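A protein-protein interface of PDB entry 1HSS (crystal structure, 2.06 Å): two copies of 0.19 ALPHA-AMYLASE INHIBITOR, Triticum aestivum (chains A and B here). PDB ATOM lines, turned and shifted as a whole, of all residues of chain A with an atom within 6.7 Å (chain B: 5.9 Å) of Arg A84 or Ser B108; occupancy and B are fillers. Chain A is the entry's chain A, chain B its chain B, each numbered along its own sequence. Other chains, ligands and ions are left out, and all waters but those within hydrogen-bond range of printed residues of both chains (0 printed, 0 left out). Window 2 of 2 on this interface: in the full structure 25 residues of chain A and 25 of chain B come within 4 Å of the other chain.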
ATOM      1  N   CYS A  28      -1.490   5.704 -25.205  1.00  0.00           N
ATOM      2  CA  CYS A  28      -2.353   6.794 -25.687  1.00  0.00           C
ATOM      3  C   CYS A  28      -2.920   6.634 -27.111  1.00  0.00           C
ATOM      4  O   CYS A  28      -3.917   7.276 -27.453  1.00  0.00           O
ATOM      5  CB  CYS A  28      -1.693   8.178 -25.515  1.00  0.00           C
ATOM      6  SG  CYS A  28      -0.252   8.528 -26.546  1.00  0.00           S
ATOM      7  N   ASN A  29      -2.410   5.660 -27.862  1.00  0.00           N
ATOM      8  CA  ASN A  29      -3.085   5.223 -29.081  1.00  0.00           C
ATOM      9  C   ASN A  29      -3.487   3.741 -29.105  1.00  0.00           C
ATOM     10  O   ASN A  29      -3.700   3.168 -30.175  1.00  0.00           O
ATOM     11  CB  ASN A  29      -2.246   5.546 -30.319  1.00  0.00           C
ATOM     12  CG  ASN A  29      -0.828   5.028 -30.223  1.00  0.00           C
ATOM     13  OD1 ASN A  29       0.100   5.631 -30.762  1.00  0.00           O
ATOM     14  ND2 ASN A  29      -0.648   3.900 -29.554  1.00  0.00           N
ATOM     15  N   TYR A  65       5.532  17.382 -22.859  1.00  0.00           N
ATOM     16  CA  TYR A  65       4.942  18.440 -23.667  1.00  0.00           C
ATOM     17  C   TYR A  65       5.860  19.614 -23.908  1.00  0.00           C
ATOM     18  O   TYR A  65       5.787  20.260 -24.949  1.00  0.00           O
ATOM     19  CB  TYR A  65       3.670  18.935 -23.012  1.00  0.00           C
ATOM     20  CG  TYR A  65       2.483  18.179 -23.486  1.00  0.00           C
ATOM     21  CD1 TYR A  65       2.265  18.000 -24.840  1.00  0.00           C
ATOM     22  CD2 TYR A  65       1.574  17.646 -22.593  1.00  0.00           C
ATOM     23  CE1 TYR A  65       1.157  17.321 -25.300  1.00  0.00           C
ATOM     24  CE2 TYR A  65       0.465  16.954 -23.041  1.00  0.00           C
ATOM     25  CZ  TYR A  65       0.255  16.807 -24.398  1.00  0.00           C
ATOM     26  OH  TYR A  65      -0.902  16.237 -24.863  1.00  0.00           O
ATOM     27  N   PHE A  80       3.442  13.224 -28.510  1.00  0.00           N
ATOM     28  CA  PHE A  80       2.653  11.991 -28.532  1.00  0.00           C
ATOM     29  C   PHE A  80       2.125  11.606 -29.906  1.00  0.00           C
ATOM     30  O   PHE A  80       1.078  12.095 -30.342  1.00  0.00           O
ATOM     31  CB  PHE A  80       1.499  12.115 -27.558  1.00  0.00           C
ATOM     32  CG  PHE A  80       1.938  12.449 -26.189  1.00  0.00           C
ATOM     33  CD1 PHE A  80       2.473  11.463 -25.377  1.00  0.00           C
ATOM     34  CD2 PHE A  80       2.003  13.770 -25.778  1.00  0.00           C
ATOM     35  CE1 PHE A  80       3.068  11.782 -24.199  1.00  0.00           C
ATOM     36  CE2 PHE A  80       2.603  14.100 -24.591  1.00  0.00           C
ATOM     37  CZ  PHE A  80       3.137  13.114 -23.799  1.00  0.00           C
ATOM     38  N   ARG A  82       0.375  10.073 -32.929  1.00  0.00           N
ATOM     39  CA  ARG A  82      -0.887   9.364 -33.158  1.00  0.00           C
ATOM     40  C   ARG A  82      -1.837   9.396 -31.956  1.00  0.00           C
ATOM     41  O   ARG A  82      -2.881   8.728 -31.964  1.00  0.00           O
ATOM     42  CB  ARG A  82      -0.625   7.914 -33.588  1.00  0.00           C
ATOM     43  CG  ARG A  82      -0.145   7.764 -35.030  1.00  0.00           C
ATOM     44  CD  ARG A  82       0.800   6.569 -35.193  1.00  0.00           C
ATOM     45  NE  ARG A  82       2.162   6.984 -35.536  1.00  0.00           N
ATOM     46  CZ  ARG A  82       3.240   6.738 -34.793  1.00  0.00           C
ATOM     47  NH1 ARG A  82       3.142   6.042 -33.661  1.00  0.00           N
ATOM     48  NH2 ARG A  82       4.426   7.182 -35.190  1.00  0.00           N
ATOM     49  N   CYS A  83      -1.558  10.299 -31.014  1.00  0.00           N
ATOM     50  CA  CYS A  83      -2.409  10.492 -29.842  1.00  0.00           C
ATOM     51  C   CYS A  83      -3.124  11.832 -29.759  1.00  0.00           C
ATOM     52  O   CYS A  83      -2.530  12.890 -29.967  1.00  0.00           O
ATOM     53  CB  CYS A  83      -1.617  10.303 -28.563  1.00  0.00           C
ATOM     54  SG  CYS A  83      -1.021   8.627 -28.416  1.00  0.00           S
ATOM     55  N   ARG A  84      -4.357  11.763 -29.273  1.00  0.00           N
ATOM     56  CA  ARG A  84      -5.169  12.937 -29.004  1.00  0.00           C
ATOM     57  C   ARG A  84      -4.864  13.547 -27.644  1.00  0.00           C
ATOM     58  O   ARG A  84      -4.863  12.853 -26.630  1.00  0.00           O
ATOM     59  CB  ARG A  84      -6.642  12.563 -29.044  1.00  0.00           C
ATOM     60  CG  ARG A  84      -7.063  11.839 -30.289  1.00  0.00           C
ATOM     61  CD  ARG A  84      -8.552  11.693 -30.315  1.00  0.00           C
ATOM     62  NE  ARG A  84      -8.950  10.930 -31.481  1.00  0.00           N
ATOM     63  CZ  ARG A  84     -10.167  10.964 -31.995  1.00  0.00           C
ATOM     64  NH1 ARG A  84     -11.096  11.717 -31.416  1.00  0.00           N
ATOM     65  NH2 ARG A  84     -10.445  10.219 -33.063  1.00  0.00           N
ATOM     66  N   ARG A  85      -4.800  14.872 -27.616  1.00  0.00           N
ATOM     67  CA  ARG A  85      -4.579  15.650 -26.397  1.00  0.00           C
ATOM     68  C   ARG A  85      -5.410  15.161 -25.205  1.00  0.00           C
ATOM     69  O   ARG A  85      -4.890  14.882 -24.134  1.00  0.00           O
ATOM     70  CB  ARG A  85      -4.904  17.121 -26.691  1.00  0.00           C
ATOM     71  CG  ARG A  85      -3.906  18.136 -26.146  1.00  0.00           C
ATOM     72  CD  ARG A  85      -4.354  18.741 -24.800  1.00  0.00           C
ATOM     73  NE  ARG A  85      -3.337  19.638 -24.235  1.00  0.00           N
ATOM     74  CZ  ARG A  85      -3.579  20.620 -23.370  1.00  0.00           C
ATOM     75  NH1 ARG A  85      -4.809  20.826 -22.904  1.00  0.00           N
ATOM     76  NH2 ARG A  85      -2.579  21.395 -22.968  1.00  0.00           N
ATOM     77  N   GLU A  86      -6.699  14.975 -25.442  1.00  0.00           N
ATOM     78  CA  GLU A  86      -7.639  14.581 -24.393  1.00  0.00           C
ATOM     79  C   GLU A  86      -7.326  13.193 -23.803  1.00  0.00           C
ATOM     80  O   GLU A  86      -7.312  13.022 -22.582  1.00  0.00           O
ATOM     81  CB  GLU A  86      -9.083  14.595 -24.935  1.00  0.00           C
ATOM     82  CG  GLU A  86      -9.351  15.554 -26.125  1.00  0.00           C
ATOM     83  CD  GLU A  86      -9.013  14.958 -27.514  1.00  0.00           C
ATOM     84  OE1 GLU A  86      -9.658  13.959 -27.935  1.00  0.00           O
ATOM     85  OE2 GLU A  86      -8.147  15.544 -28.217  1.00  0.00           O
ATOM     86  N   VAL A  87      -7.051  12.216 -24.675  1.00  0.00           N
ATOM     87  CA  VAL A  87      -6.787  10.855 -24.223  1.00  0.00           C
ATOM     88  C   VAL A  87      -5.394  10.739 -23.609  1.00  0.00           C
ATOM     89  O   VAL A  87      -5.221  10.038 -22.620  1.00  0.00           O
ATOM     90  CB  VAL A  87      -6.975   9.789 -25.355  1.00  0.00           C
ATOM     91  CG1 VAL A  87      -8.139  10.158 -26.264  1.00  0.00           C
ATOM     92  CG2 VAL A  87      -5.726   9.643 -26.147  1.00  0.00           C
ATOM     93  N   VAL A  88      -4.457  11.556 -24.084  1.00  0.00           N
ATOM     94  CA  VAL A  88      -3.127  11.622 -23.484  1.00  0.00           C
ATOM     95  C   VAL A  88      -3.187  11.982 -21.995  1.00  0.00           C
ATOM     96  O   VAL A  88      -2.654  11.255 -21.164  1.00  0.00           O
ATOM     97  CB  VAL A  88      -2.184  12.630 -24.237  1.00  0.00           C
ATOM     98  CG1 VAL A  88      -0.943  12.953 -23.404  1.00  0.00           C
ATOM     99  CG2 VAL A  88      -1.744  12.043 -25.556  1.00  0.00           C
ATOM    100  N   LYS A  89      -3.898  13.040 -21.630  1.00  0.00           N
ATOM    101  CA  LYS A  89      -3.871  13.455 -20.229  1.00  0.00           C
ATOM    102  C   LYS A  89      -4.793  12.612 -19.374  1.00  0.00           C
ATOM    103  O   LYS A  89      -4.509  12.402 -18.202  1.00  0.00           O
ATOM    104  CB  LYS A  89      -4.179  14.950 -20.058  1.00  0.00           C
ATOM    105  CG  LYS A  89      -5.531  15.355 -20.556  1.00  0.00           C
ATOM    106  CD  LYS A  89      -5.773  16.841 -20.344  1.00  0.00           C
ATOM    107  CE  LYS A  89      -5.299  17.649 -21.540  1.00  0.00           C
ATOM    108  NZ  LYS A  89      -3.886  17.293 -21.903  1.00  0.00           N
ATOM    109  N   TRP B  51     -15.457  -1.226 -29.885  1.00  0.00           N
ATOM    110  CA  TRP B  51     -16.264  -0.082 -30.243  1.00  0.00           C
ATOM    111  C   TRP B  51     -17.300   0.239 -29.185  1.00  0.00           C
ATOM    112  O   TRP B  51     -17.846   1.333 -29.174  1.00  0.00           O
ATOM    113  CB  TRP B  51     -16.966  -0.339 -31.578  1.00  0.00           C
ATOM    114  CG  TRP B  51     -16.030  -0.502 -32.723  1.00  0.00           C
ATOM    115  CD1 TRP B  51     -15.167  -1.546 -32.936  1.00  0.00           C
ATOM    116  CD2 TRP B  51     -15.759   0.462 -33.750  1.00  0.00           C
ATOM    117  NE1 TRP B  51     -14.357  -1.274 -34.016  1.00  0.00           N
ATOM    118  CE2 TRP B  51     -14.708  -0.053 -34.541  1.00  0.00           C
ATOM    119  CE3 TRP B  51     -16.286   1.718 -34.065  1.00  0.00           C
ATOM    120  CZ2 TRP B  51     -14.183   0.645 -35.633  1.00  0.00           C
ATOM    121  CZ3 TRP B  51     -15.759   2.411 -35.143  1.00  0.00           C
ATOM    122  CH2 TRP B  51     -14.722   1.872 -35.915  1.00  0.00           C
ATOM    123  N   VAL B 105     -11.727   5.036 -30.214  1.00  0.00           N
ATOM    124  CA  VAL B 105     -12.105   6.362 -29.729  1.00  0.00           C
ATOM    125  C   VAL B 105     -13.277   6.900 -30.514  1.00  0.00           C
ATOM    126  O   VAL B 105     -14.194   7.486 -29.939  1.00  0.00           O
ATOM    127  CB  VAL B 105     -10.941   7.387 -29.816  1.00  0.00           C
ATOM    128  CG1 VAL B 105     -11.379   8.694 -29.235  1.00  0.00           C
ATOM    129  CG2 VAL B 105      -9.737   6.896 -29.060  1.00  0.00           C
ATOM    130  N   ASP B 106     -13.238   6.712 -31.831  1.00  0.00           N
ATOM    131  CA  ASP B 106     -14.399   6.997 -32.663  1.00  0.00           C
ATOM    132  C   ASP B 106     -14.303   6.395 -34.051  1.00  0.00           C
ATOM    133  O   ASP B 106     -13.522   5.476 -34.284  1.00  0.00           O
ATOM    134  CB  ASP B 106     -14.656   8.513 -32.753  1.00  0.00           C
ATOM    135  CG  ASP B 106     -13.469   9.293 -33.302  1.00  0.00           C
ATOM    136  OD1 ASP B 106     -12.612   8.720 -34.021  1.00  0.00           O
ATOM    137  OD2 ASP B 106     -13.421  10.514 -33.019  1.00  0.00           O
ATOM    138  N   ALA B 107     -15.020   7.016 -34.984  1.00  0.00           N
ATOM    139  CA  ALA B 107     -15.225   6.490 -36.332  1.00  0.00           C
ATOM    140  C   ALA B 107     -13.931   6.335 -37.148  1.00  0.00           C
ATOM    141  O   ALA B 107     -13.850   5.474 -38.020  1.00  0.00           O
ATOM    142  CB  ALA B 107     -16.226   7.380 -37.078  1.00  0.00           C
ATOM    143  N   SER B 108     -12.915   7.135 -36.827  1.00  0.00           N
ATOM    144  CA  SER B 108     -11.577   6.978 -37.409  1.00  0.00           C
ATOM    145  C   SER B 108     -10.972   5.577 -37.205  1.00  0.00           C
ATOM    146  O   SER B 108     -10.154   5.124 -38.005  1.00  0.00           O
ATOM    147  CB  SER B 108     -10.626   8.019 -36.807  1.00  0.00           C
ATOM    148  OG  SER B 108     -10.574   7.919 -35.385  1.00  0.00           O
ATOM    149  N   GLY B 109     -11.333   4.917 -36.106  1.00  0.00           N
ATOM    150  CA  GLY B 109     -10.663   3.679 -35.721  1.00  0.00           C
ATOM    151  C   GLY B 109      -9.455   3.911 -34.814  1.00  0.00           C
ATOM    152  O   GLY B 109      -8.659   2.995 -34.564  1.00  0.00           O
ATOM    153  N   ASP B 110      -9.273   5.167 -34.402  1.00  0.00           N
ATOM    154  CA  ASP B 110      -8.231   5.531 -33.448  1.00  0.00           C
ATOM    155  C   ASP B 110      -8.439   4.732 -32.170  1.00  0.00           C
ATOM    156  O   ASP B 110      -9.551   4.656 -31.659  1.00  0.00           O
ATOM    157  CB  ASP B 110      -8.296   7.034 -33.116  1.00  0.00           C
ATOM    158  CG  ASP B 110      -7.660   7.920 -34.191  1.00  0.00           C
ATOM    159  OD1 ASP B 110      -7.016   7.389 -35.136  1.00  0.00           O
ATOM    160  OD2 ASP B 110      -7.821   9.164 -34.078  1.00  0.00           O
ATOM    161  N   LYS B 116     -13.091   8.837 -22.834  1.00  0.00           N
ATOM    162  CA  LYS B 116     -13.250  10.271 -22.600  1.00  0.00           C
ATOM    163  C   LYS B 116     -14.720  10.704 -22.429  1.00  0.00           C
ATOM    164  O   LYS B 116     -15.047  11.568 -21.594  1.00  0.00           O
ATOM    165  CB  LYS B 116     -12.559  11.074 -23.722  1.00  0.00           C
ATOM    166  CG  LYS B 116     -13.108  10.850 -25.136  1.00  0.00           C
ATOM    167  CD  LYS B 116     -12.442  11.758 -26.152  1.00  0.00           C
ATOM    168  CE  LYS B 116     -12.958  11.502 -27.561  1.00  0.00           C
ATOM    169  NZ  LYS B 116     -14.184  12.304 -27.826  1.00  0.00           N
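Arg A84 touches just these residues of chain B: Val B105, Asp B106, Ser B108 and Asp B110. Ser B108 touches just one residue of chain A: Arg A84 (3.3 Å). Printed residues of chain A within 4 Å of Asp B110: Arg A84. Of the printed residues of chain A, Val B105 touches Arg A84 (3.7 Å). Of the printed residues of chain A, Asp B106 touches Arg A84. Of the printed residues of chain A, Lys B116 touches Glu A86 (3.97 Å). Asn A29 touches none of the printed residues of chain B. The nearest residue of chain B that does not touch Arg A84 is Lys B116 (4.3 Å).
Among the printed residues, merely in contact across the chains: Arg A84 with Val B105 (3.7 Å) and Glu A86 with Lys B116 (3.97 Å).
OG of Ser B108 sits close to N of Asp B110, 3.2 Å away. The side-chain sulfur (SG) of Cys A83 forms a disulfide with the side-chain sulfur (SG) of Cys A28 (2.0 Å). The backbone NH (N) of Val B105 lies within hydrogen-bond range of the backbone carbonyl oxygen (O) of Asp B110, 2.6 Å away. The side-chain hydroxyl of Ser B108 is in hydrogen-bond range of the side-chain carboxylate of Asp B106.
No position is printed for both chains. Of the 5 pairs that touch across the chains among the printed residues, none has its exchanged pair printed and touching as well.
NH2 of Arg A84 lies within salt-bridge range of OD1 of Asp B106 (2.8 Å). The side-chain hydroxyl (OG) of Ser B108 sits at hydrogen-bond distance from the guanidinium group (NH2) of Arg A84, 3.3 Å away. The guanidinium group (NH2) of Arg A84 lies within salt-bridge range of the side-chain carboxylate (OD2) of Asp B110 (3.0 Å).
Of the 8 printed residues of chain B, 5 touch a printed residue of chain A. Hydrophobic or aromatic side chains of chain B that line the printed part of chain A: Val B105. Among the printed residues, 5 pairs touch across the chains.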
